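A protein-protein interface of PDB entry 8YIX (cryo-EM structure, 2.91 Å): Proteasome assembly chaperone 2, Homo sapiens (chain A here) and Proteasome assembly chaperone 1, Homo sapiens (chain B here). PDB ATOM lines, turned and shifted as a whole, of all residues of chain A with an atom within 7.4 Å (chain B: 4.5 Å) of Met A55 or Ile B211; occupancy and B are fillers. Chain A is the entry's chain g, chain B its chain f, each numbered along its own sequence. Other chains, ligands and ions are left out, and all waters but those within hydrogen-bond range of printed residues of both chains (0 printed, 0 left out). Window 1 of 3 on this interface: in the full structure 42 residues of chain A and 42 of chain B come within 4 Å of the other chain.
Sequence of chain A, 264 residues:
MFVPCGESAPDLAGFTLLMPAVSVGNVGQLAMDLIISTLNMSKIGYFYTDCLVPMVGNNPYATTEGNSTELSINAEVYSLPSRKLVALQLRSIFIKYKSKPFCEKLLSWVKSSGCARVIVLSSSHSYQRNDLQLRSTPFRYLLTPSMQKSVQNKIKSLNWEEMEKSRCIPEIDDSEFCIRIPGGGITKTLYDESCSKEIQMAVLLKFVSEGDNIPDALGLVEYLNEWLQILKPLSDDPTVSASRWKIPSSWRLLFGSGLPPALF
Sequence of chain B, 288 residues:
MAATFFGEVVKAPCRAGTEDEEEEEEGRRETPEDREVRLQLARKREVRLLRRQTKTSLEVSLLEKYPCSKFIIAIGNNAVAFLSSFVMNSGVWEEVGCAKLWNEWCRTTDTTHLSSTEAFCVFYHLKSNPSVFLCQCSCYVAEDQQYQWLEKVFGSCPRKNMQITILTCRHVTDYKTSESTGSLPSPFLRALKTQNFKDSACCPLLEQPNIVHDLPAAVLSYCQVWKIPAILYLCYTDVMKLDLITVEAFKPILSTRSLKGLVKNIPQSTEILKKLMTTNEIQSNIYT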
ATOM      1  N   LEU A  52      27.156 -15.999 -20.906  1.00  0.00           N
ATOM      2  CA  LEU A  52      26.270 -17.151 -20.951  1.00  0.00           C
ATOM      3  C   LEU A  52      24.830 -16.676 -20.904  1.00  0.00           C
ATOM      4  O   LEU A  52      24.514 -15.723 -20.194  1.00  0.00           O
ATOM      5  CB  LEU A  52      26.539 -18.095 -19.779  1.00  0.00           C
ATOM      6  CG  LEU A  52      27.652 -19.126 -19.824  1.00  0.00           C
ATOM      7  CD1 LEU A  52      28.093 -19.370 -18.438  1.00  0.00           C
ATOM      8  CD2 LEU A  52      27.164 -20.400 -20.399  1.00  0.00           C
ATOM      9  N   VAL A  53      23.965 -17.338 -21.662  1.00  0.00           N
ATOM     10  CA  VAL A  53      22.541 -16.994 -21.648  1.00  0.00           C
ATOM     11  C   VAL A  53      22.026 -17.117 -20.225  1.00  0.00           C
ATOM     12  O   VAL A  53      22.239 -18.162 -19.586  1.00  0.00           O
ATOM     13  CB  VAL A  53      21.757 -17.915 -22.594  1.00  0.00           C
ATOM     14  CG1 VAL A  53      20.302 -17.566 -22.588  1.00  0.00           C
ATOM     15  CG2 VAL A  53      22.304 -17.814 -23.981  1.00  0.00           C
ATOM     16  N   PRO A  54      21.384 -16.095 -19.663  1.00  0.00           N
ATOM     17  CA  PRO A  54      20.991 -16.168 -18.254  1.00  0.00           C
ATOM     18  C   PRO A  54      19.880 -17.172 -18.030  1.00  0.00           C
ATOM     19  O   PRO A  54      18.992 -17.339 -18.863  1.00  0.00           O
ATOM     20  CB  PRO A  54      20.537 -14.742 -17.944  1.00  0.00           C
ATOM     21  CG  PRO A  54      20.189 -14.174 -19.232  1.00  0.00           C
ATOM     22  CD  PRO A  54      21.078 -14.784 -20.244  1.00  0.00           C
ATOM     23  N   MET A  55      19.954 -17.858 -16.898  1.00  0.00           N
ATOM     24  CA  MET A  55      18.957 -18.832 -16.497  1.00  0.00           C
ATOM     25  C   MET A  55      18.980 -18.900 -14.986  1.00  0.00           C
ATOM     26  O   MET A  55      19.921 -18.432 -14.344  1.00  0.00           O
ATOM     27  CB  MET A  55      19.207 -20.207 -17.126  1.00  0.00           C
ATOM     28  CG  MET A  55      20.521 -20.875 -16.775  1.00  0.00           C
ATOM     29  SD  MET A  55      20.620 -21.687 -15.180  1.00  0.00           S
ATOM     30  CE  MET A  55      19.570 -23.073 -15.469  1.00  0.00           C
ATOM     31  N   VAL A  56      17.920 -19.463 -14.413  1.00  0.00           N
ATOM     32  CA  VAL A  56      17.780 -19.487 -12.966  1.00  0.00           C
ATOM     33  C   VAL A  56      16.837 -20.622 -12.593  1.00  0.00           C
ATOM     34  O   VAL A  56      15.927 -20.964 -13.344  1.00  0.00           O
ATOM     35  CB  VAL A  56      17.296 -18.108 -12.441  1.00  0.00           C
ATOM     36  CG1 VAL A  56      15.838 -17.878 -12.732  1.00  0.00           C
ATOM     37  CG2 VAL A  56      17.587 -17.957 -11.008  1.00  0.00           C
ATOM     38  N   GLY A  57      17.096 -21.234 -11.449  1.00  0.00           N
ATOM     39  CA  GLY A  57      16.240 -22.271 -10.917  1.00  0.00           C
ATOM     40  C   GLY A  57      16.737 -22.652  -9.544  1.00  0.00           C
ATOM     41  O   GLY A  57      17.891 -22.394  -9.199  1.00  0.00           O
ATOM     42  N   ASN A  58      15.859 -23.278  -8.767  1.00  0.00           N
ATOM     43  CA  ASN A  58      16.209 -23.615  -7.395  1.00  0.00           C
ATOM     44  C   ASN A  58      17.343 -24.633  -7.376  1.00  0.00           C
ATOM     45  O   ASN A  58      17.786 -25.127  -8.407  1.00  0.00           O
ATOM     46  CB  ASN A  58      15.001 -24.153  -6.640  1.00  0.00           C
ATOM     47  CG  ASN A  58      14.082 -23.070  -6.153  1.00  0.00           C
ATOM     48  OD1 ASN A  58      14.515 -21.992  -5.774  1.00  0.00           O
ATOM     49  ND2 ASN A  58      12.798 -23.359  -6.141  1.00  0.00           N
ATOM     50  N   LEU A  71      18.331 -20.619  -4.584  1.00  0.00           N
ATOM     51  CA  LEU A  71      18.360 -20.229  -5.986  1.00  0.00           C
ATOM     52  C   LEU A  71      19.733 -20.460  -6.599  1.00  0.00           C
ATOM     53  O   LEU A  71      20.762 -20.307  -5.944  1.00  0.00           O
ATOM     54  CB  LEU A  71      17.977 -18.765  -6.123  1.00  0.00           C
ATOM     55  CG  LEU A  71      17.584 -18.300  -7.513  1.00  0.00           C
ATOM     56  CD1 LEU A  71      16.255 -18.876  -7.901  1.00  0.00           C
ATOM     57  CD2 LEU A  71      17.550 -16.810  -7.538  1.00  0.00           C
ATOM     58  N   SER A  72      19.742 -20.828  -7.876  1.00  0.00           N
ATOM     59  CA  SER A  72      20.971 -21.050  -8.620  1.00  0.00           C
ATOM     60  C   SER A  72      20.919 -20.340  -9.962  1.00  0.00           C
ATOM     61  O   SER A  72      19.879 -20.285 -10.607  1.00  0.00           O
ATOM     62  CB  SER A  72      21.225 -22.527  -8.854  1.00  0.00           C
ATOM     63  OG  SER A  72      21.432 -23.198  -7.630  1.00  0.00           O
ATOM     64  N   ILE A  73      22.069 -19.826 -10.385  1.00  0.00           N
ATOM     65  CA  ILE A  73      22.192 -19.104 -11.645  1.00  0.00           C
ATOM     66  C   ILE A  73      23.070 -19.914 -12.593  1.00  0.00           C
ATOM     67  O   ILE A  73      23.476 -21.029 -12.268  1.00  0.00           O
ATOM     68  CB  ILE A  73      22.734 -17.686 -11.410  1.00  0.00           C
ATOM     69  CG1 ILE A  73      24.239 -17.712 -11.169  1.00  0.00           C
ATOM     70  CG2 ILE A  73      22.033 -17.061 -10.235  1.00  0.00           C
ATOM     71  CD1 ILE A  73      24.913 -16.402 -11.422  1.00  0.00           C
ATOM     72  N   ASN A  74      23.342 -19.384 -13.786  1.00  0.00           N
ATOM     73  CA  ASN A  74      23.911 -20.227 -14.832  1.00  0.00           C
ATOM     74  C   ASN A  74      25.366 -20.596 -14.584  1.00  0.00           C
ATOM     75  O   ASN A  74      25.824 -21.618 -15.096  1.00  0.00           O
ATOM     76  CB  ASN A  74      23.770 -19.570 -16.203  1.00  0.00           C
ATOM     77  CG  ASN A  74      24.253 -18.162 -16.232  1.00  0.00           C
ATOM     78  OD1 ASN A  74      24.862 -17.684 -15.292  1.00  0.00           O
ATOM     79  ND2 ASN A  74      23.988 -17.480 -17.319  1.00  0.00           N
ATOM     80  N   ALA A  75      26.119 -19.802 -13.828  1.00  0.00           N
ATOM     81  CA  ALA A  75      27.523 -20.109 -13.558  1.00  0.00           C
ATOM     82  C   ALA A  75      27.808 -19.911 -12.080  1.00  0.00           C
ATOM     83  O   ALA A  75      27.786 -18.781 -11.591  1.00  0.00           O
ATOM     84  CB  ALA A  75      28.439 -19.246 -14.413  1.00  0.00           C
ATOM     85  N   LEU A  90      28.853 -24.516 -15.237  1.00  0.00           N
ATOM     86  CA  LEU A  90      28.167 -23.677 -16.206  1.00  0.00           C
ATOM     87  C   LEU A  90      26.892 -24.392 -16.619  1.00  0.00           C
ATOM     88  O   LEU A  90      26.948 -25.517 -17.112  1.00  0.00           O
ATOM     89  CB  LEU A  90      29.048 -23.436 -17.425  1.00  0.00           C
ATOM     90  CG  LEU A  90      30.504 -23.026 -17.266  1.00  0.00           C
ATOM     91  CD1 LEU A  90      31.144 -23.019 -18.621  1.00  0.00           C
ATOM     92  CD2 LEU A  90      30.611 -21.678 -16.626  1.00  0.00           C
ATOM     93  N   ARG A  91      25.749 -23.749 -16.433  1.00  0.00           N
ATOM     94  CA  ARG A  91      24.473 -24.415 -16.636  1.00  0.00           C
ATOM     95  C   ARG A  91      23.699 -23.858 -17.818  1.00  0.00           C
ATOM     96  O   ARG A  91      22.497 -24.093 -17.929  1.00  0.00           O
ATOM     97  CB  ARG A  91      23.631 -24.331 -15.370  1.00  0.00           C
ATOM     98  CG  ARG A  91      23.911 -25.422 -14.403  1.00  0.00           C
ATOM     99  CD  ARG A  91      23.079 -25.279 -13.188  1.00  0.00           C
ATOM    100  NE  ARG A  91      23.690 -24.354 -12.254  1.00  0.00           N
ATOM    101  CZ  ARG A  91      24.302 -24.724 -11.142  1.00  0.00           C
ATOM    102  NH1 ARG A  91      24.380 -25.999 -10.823  1.00  0.00           N
ATOM    103  NH2 ARG A  91      24.822 -23.813 -10.348  1.00  0.00           N
ATOM    104  N   SER A  92      24.362 -23.154 -18.722  1.00  0.00           N
ATOM    105  CA  SER A  92      23.685 -22.452 -19.794  1.00  0.00           C
ATOM    106  C   SER A  92      24.479 -22.666 -21.071  1.00  0.00           C
ATOM    107  O   SER A  92      25.284 -23.591 -21.171  1.00  0.00           O
ATOM    108  CB  SER A  92      23.529 -20.972 -19.440  1.00  0.00           C
ATOM    109  OG  SER A  92      22.564 -20.348 -20.252  1.00  0.00           O
ATOM    110  N   ILE A  93      24.231 -21.824 -22.061  1.00  0.00           N
ATOM    111  CA  ILE A  93      24.919 -21.862 -23.343  1.00  0.00           C
ATOM    112  C   ILE A  93      25.496 -20.485 -23.628  1.00  0.00           C
ATOM    113  O   ILE A  93      25.024 -19.479 -23.100  1.00  0.00           O
ATOM    114  CB  ILE A  93      23.960 -22.319 -24.452  1.00  0.00           C
ATOM    115  CG1 ILE A  93      22.643 -21.589 -24.293  1.00  0.00           C
ATOM    116  CG2 ILE A  93      23.742 -23.792 -24.384  1.00  0.00           C
ATOM    117  CD1 ILE A  93      21.649 -21.948 -25.281  1.00  0.00           C
ATOM    118  N   PRO B 209      13.852 -29.585 -11.407  1.00  0.00           N
ATOM    119  CA  PRO B 209      14.263 -29.740 -12.806  1.00  0.00           C
ATOM    120  C   PRO B 209      13.825 -28.592 -13.683  1.00  0.00           C
ATOM    121  O   PRO B 209      14.317 -28.472 -14.809  1.00  0.00           O
ATOM    122  CB  PRO B 209      13.590 -31.042 -13.225  1.00  0.00           C
ATOM    123  CG  PRO B 209      12.394 -31.081 -12.428  1.00  0.00           C
ATOM    124  CD  PRO B 209      12.723 -30.470 -11.095  1.00  0.00           C
ATOM    125  N   ASN B 210      12.928 -27.745 -13.196  1.00  0.00           N
ATOM    126  CA  ASN B 210      12.426 -26.602 -13.934  1.00  0.00           C
ATOM    127  C   ASN B 210      13.344 -25.410 -13.756  1.00  0.00           C
ATOM    128  O   ASN B 210      13.799 -25.123 -12.650  1.00  0.00           O
ATOM    129  CB  ASN B 210      11.027 -26.230 -13.456  1.00  0.00           C
ATOM    130  CG  ASN B 210       9.978 -27.156 -13.959  1.00  0.00           C
ATOM    131  OD1 ASN B 210       9.549 -27.050 -15.094  1.00  0.00           O
ATOM    132  ND2 ASN B 210       9.547 -28.069 -13.117  1.00  0.00           N
ATOM    133  N   ILE B 211      13.602 -24.707 -14.855  1.00  0.00           N
ATOM    134  CA  ILE B 211      14.407 -23.498 -14.872  1.00  0.00           C
ATOM    135  C   ILE B 211      13.631 -22.427 -15.620  1.00  0.00           C
ATOM    136  O   ILE B 211      12.649 -22.704 -16.302  1.00  0.00           O
ATOM    137  CB  ILE B 211      15.790 -23.707 -15.524  1.00  0.00           C
ATOM    138  CG1 ILE B 211      15.628 -24.107 -16.984  1.00  0.00           C
ATOM    139  CG2 ILE B 211      16.571 -24.750 -14.787  1.00  0.00           C
ATOM    140  CD1 ILE B 211      16.817 -23.835 -17.821  1.00  0.00           C
ATOM    141  N   VAL B 212      14.079 -21.186 -15.468  1.00  0.00           N
ATOM    142  CA  VAL B 212      13.557 -20.045 -16.205  1.00  0.00           C
ATOM    143  C   VAL B 212      14.730 -19.370 -16.893  1.00  0.00           C
ATOM    144  O   VAL B 212      15.787 -19.191 -16.286  1.00  0.00           O
ATOM    145  CB  VAL B 212      12.819 -19.062 -15.277  1.00  0.00           C
ATOM    146  CG1 VAL B 212      12.214 -17.941 -16.057  1.00  0.00           C
ATOM    147  CG2 VAL B 212      11.759 -19.779 -14.529  1.00  0.00           C
ATOM    148  N   HIS B 213      14.564 -19.022 -18.174  1.00  0.00           N
ATOM    149  CA  HIS B 213      15.685 -18.558 -18.984  1.00  0.00           C
ATOM    150  C   HIS B 213      15.269 -17.407 -19.898  1.00  0.00           C
ATOM    151  O   HIS B 213      14.939 -17.603 -21.061  1.00  0.00           O
ATOM    152  CB  HIS B 213      16.231 -19.711 -19.811  1.00  0.00           C
ATOM    153  CG  HIS B 213      15.333 -20.103 -20.941  1.00  0.00           C
ATOM    154  ND1 HIS B 213      15.423 -19.521 -22.186  1.00  0.00           N
ATOM    155  CD2 HIS B 213      14.282 -20.951 -20.998  1.00  0.00           C
ATOM    156  CE1 HIS B 213      14.490 -20.022 -22.970  1.00  0.00           C
ATOM    157  NE2 HIS B 213      13.785 -20.894 -22.276  1.00  0.00           N
ATOM    158  N   ALA B 217      14.964 -14.216 -15.929  1.00  0.00           N
ATOM    159  CA  ALA B 217      16.122 -14.895 -15.372  1.00  0.00           C
ATOM    160  C   ALA B 217      17.319 -13.976 -15.269  1.00  0.00           C
ATOM    161  O   ALA B 217      18.113 -14.111 -14.342  1.00  0.00           O
ATOM    162  CB  ALA B 217      16.472 -16.103 -16.216  1.00  0.00           C
ATOM    163  N   SER B 221      18.911 -13.318 -11.700  1.00  0.00           N
ATOM    164  CA  SER B 221      20.326 -13.624 -11.533  1.00  0.00           C
ATOM    165  C   SER B 221      21.109 -12.413 -11.063  1.00  0.00           C
ATOM    166  O   SER B 221      21.981 -12.533 -10.199  1.00  0.00           O
ATOM    167  CB  SER B 221      20.895 -14.141 -12.840  1.00  0.00           C
ATOM    168  OG  SER B 221      20.263 -15.342 -13.212  1.00  0.00           O
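The backbone NH (N) of Val B212 lies within hydrogen-bond range of the backbone carbonyl oxygen (O) of Val A56 (2.8 Å).
The side-chain hydroxyl (OG) of Ser B221 is in hydrogen-bond range of the backbone carbonyl oxygen (O) of Met A55 (3.3 Å).
O of Ala B217 is in hydrogen-bond range of OG of Ser B221 (2.7 Å).
The backbone carbonyl oxygen (O) of Ile A73 sits at hydrogen-bond distance from the guanidinium group (NE) of Arg A91, 3.3 Å away.
Among the printed residues, merely in contact across the chains: Pro A54 with His B213 (3.5 Å), Pro A54 with Ala B217 (3.9 Å), Met A55 with Ile B211 (3.5 Å), Met A55 with Val B212 (3.2 Å), Met A55 with Ala B217 (3.7 Å), Val A56 with Ile B211 (3.3 Å), Val A56 with Ala B217 (3.96 Å) and Ile A73 with Ser B221 (3.9 Å).
Of chain B, only Ile B211 (3.5 Å), Val B212 (3.2 Å), Ala B217 (3.7 Å) and Ser B221 (3.3 Å) come within 4 Å of Met A55.
Ile B211 touches just these residues of chain A: Met A55 (3.5 Å) and Val A56 (3.3 Å).
Of the printed residues of chain B, Ile A73 touches Ser B221.
Printed residues of chain A within 4 Å of His B213: Pro A54 (3.5 Å).
Of the printed residues of chain B, Pro A54 touches His B213 and Ala B217.
Printed residues of chain A within 4 Å of Ala B217: Pro A54, Met A55 and Val A56.
Ile A93 touches none of the printed residues of chain B.
The nearest residue of chain B that does not touch Met A55 is His B213 (4.04 Å).
Hydrophobic or aromatic side chains of chain A within 4 Å of the printed part of chain B: Met A55, Val A56 and Ile A73.
Hydrophobic or aromatic side chains of chain B that line the printed part of chain A: Ile B211, His B213 and Ala B217.
Among the printed residues, no Asp or Glu carboxylate lies within 4 Å of a Lys or Arg side-chain nitrogen of the other chain.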
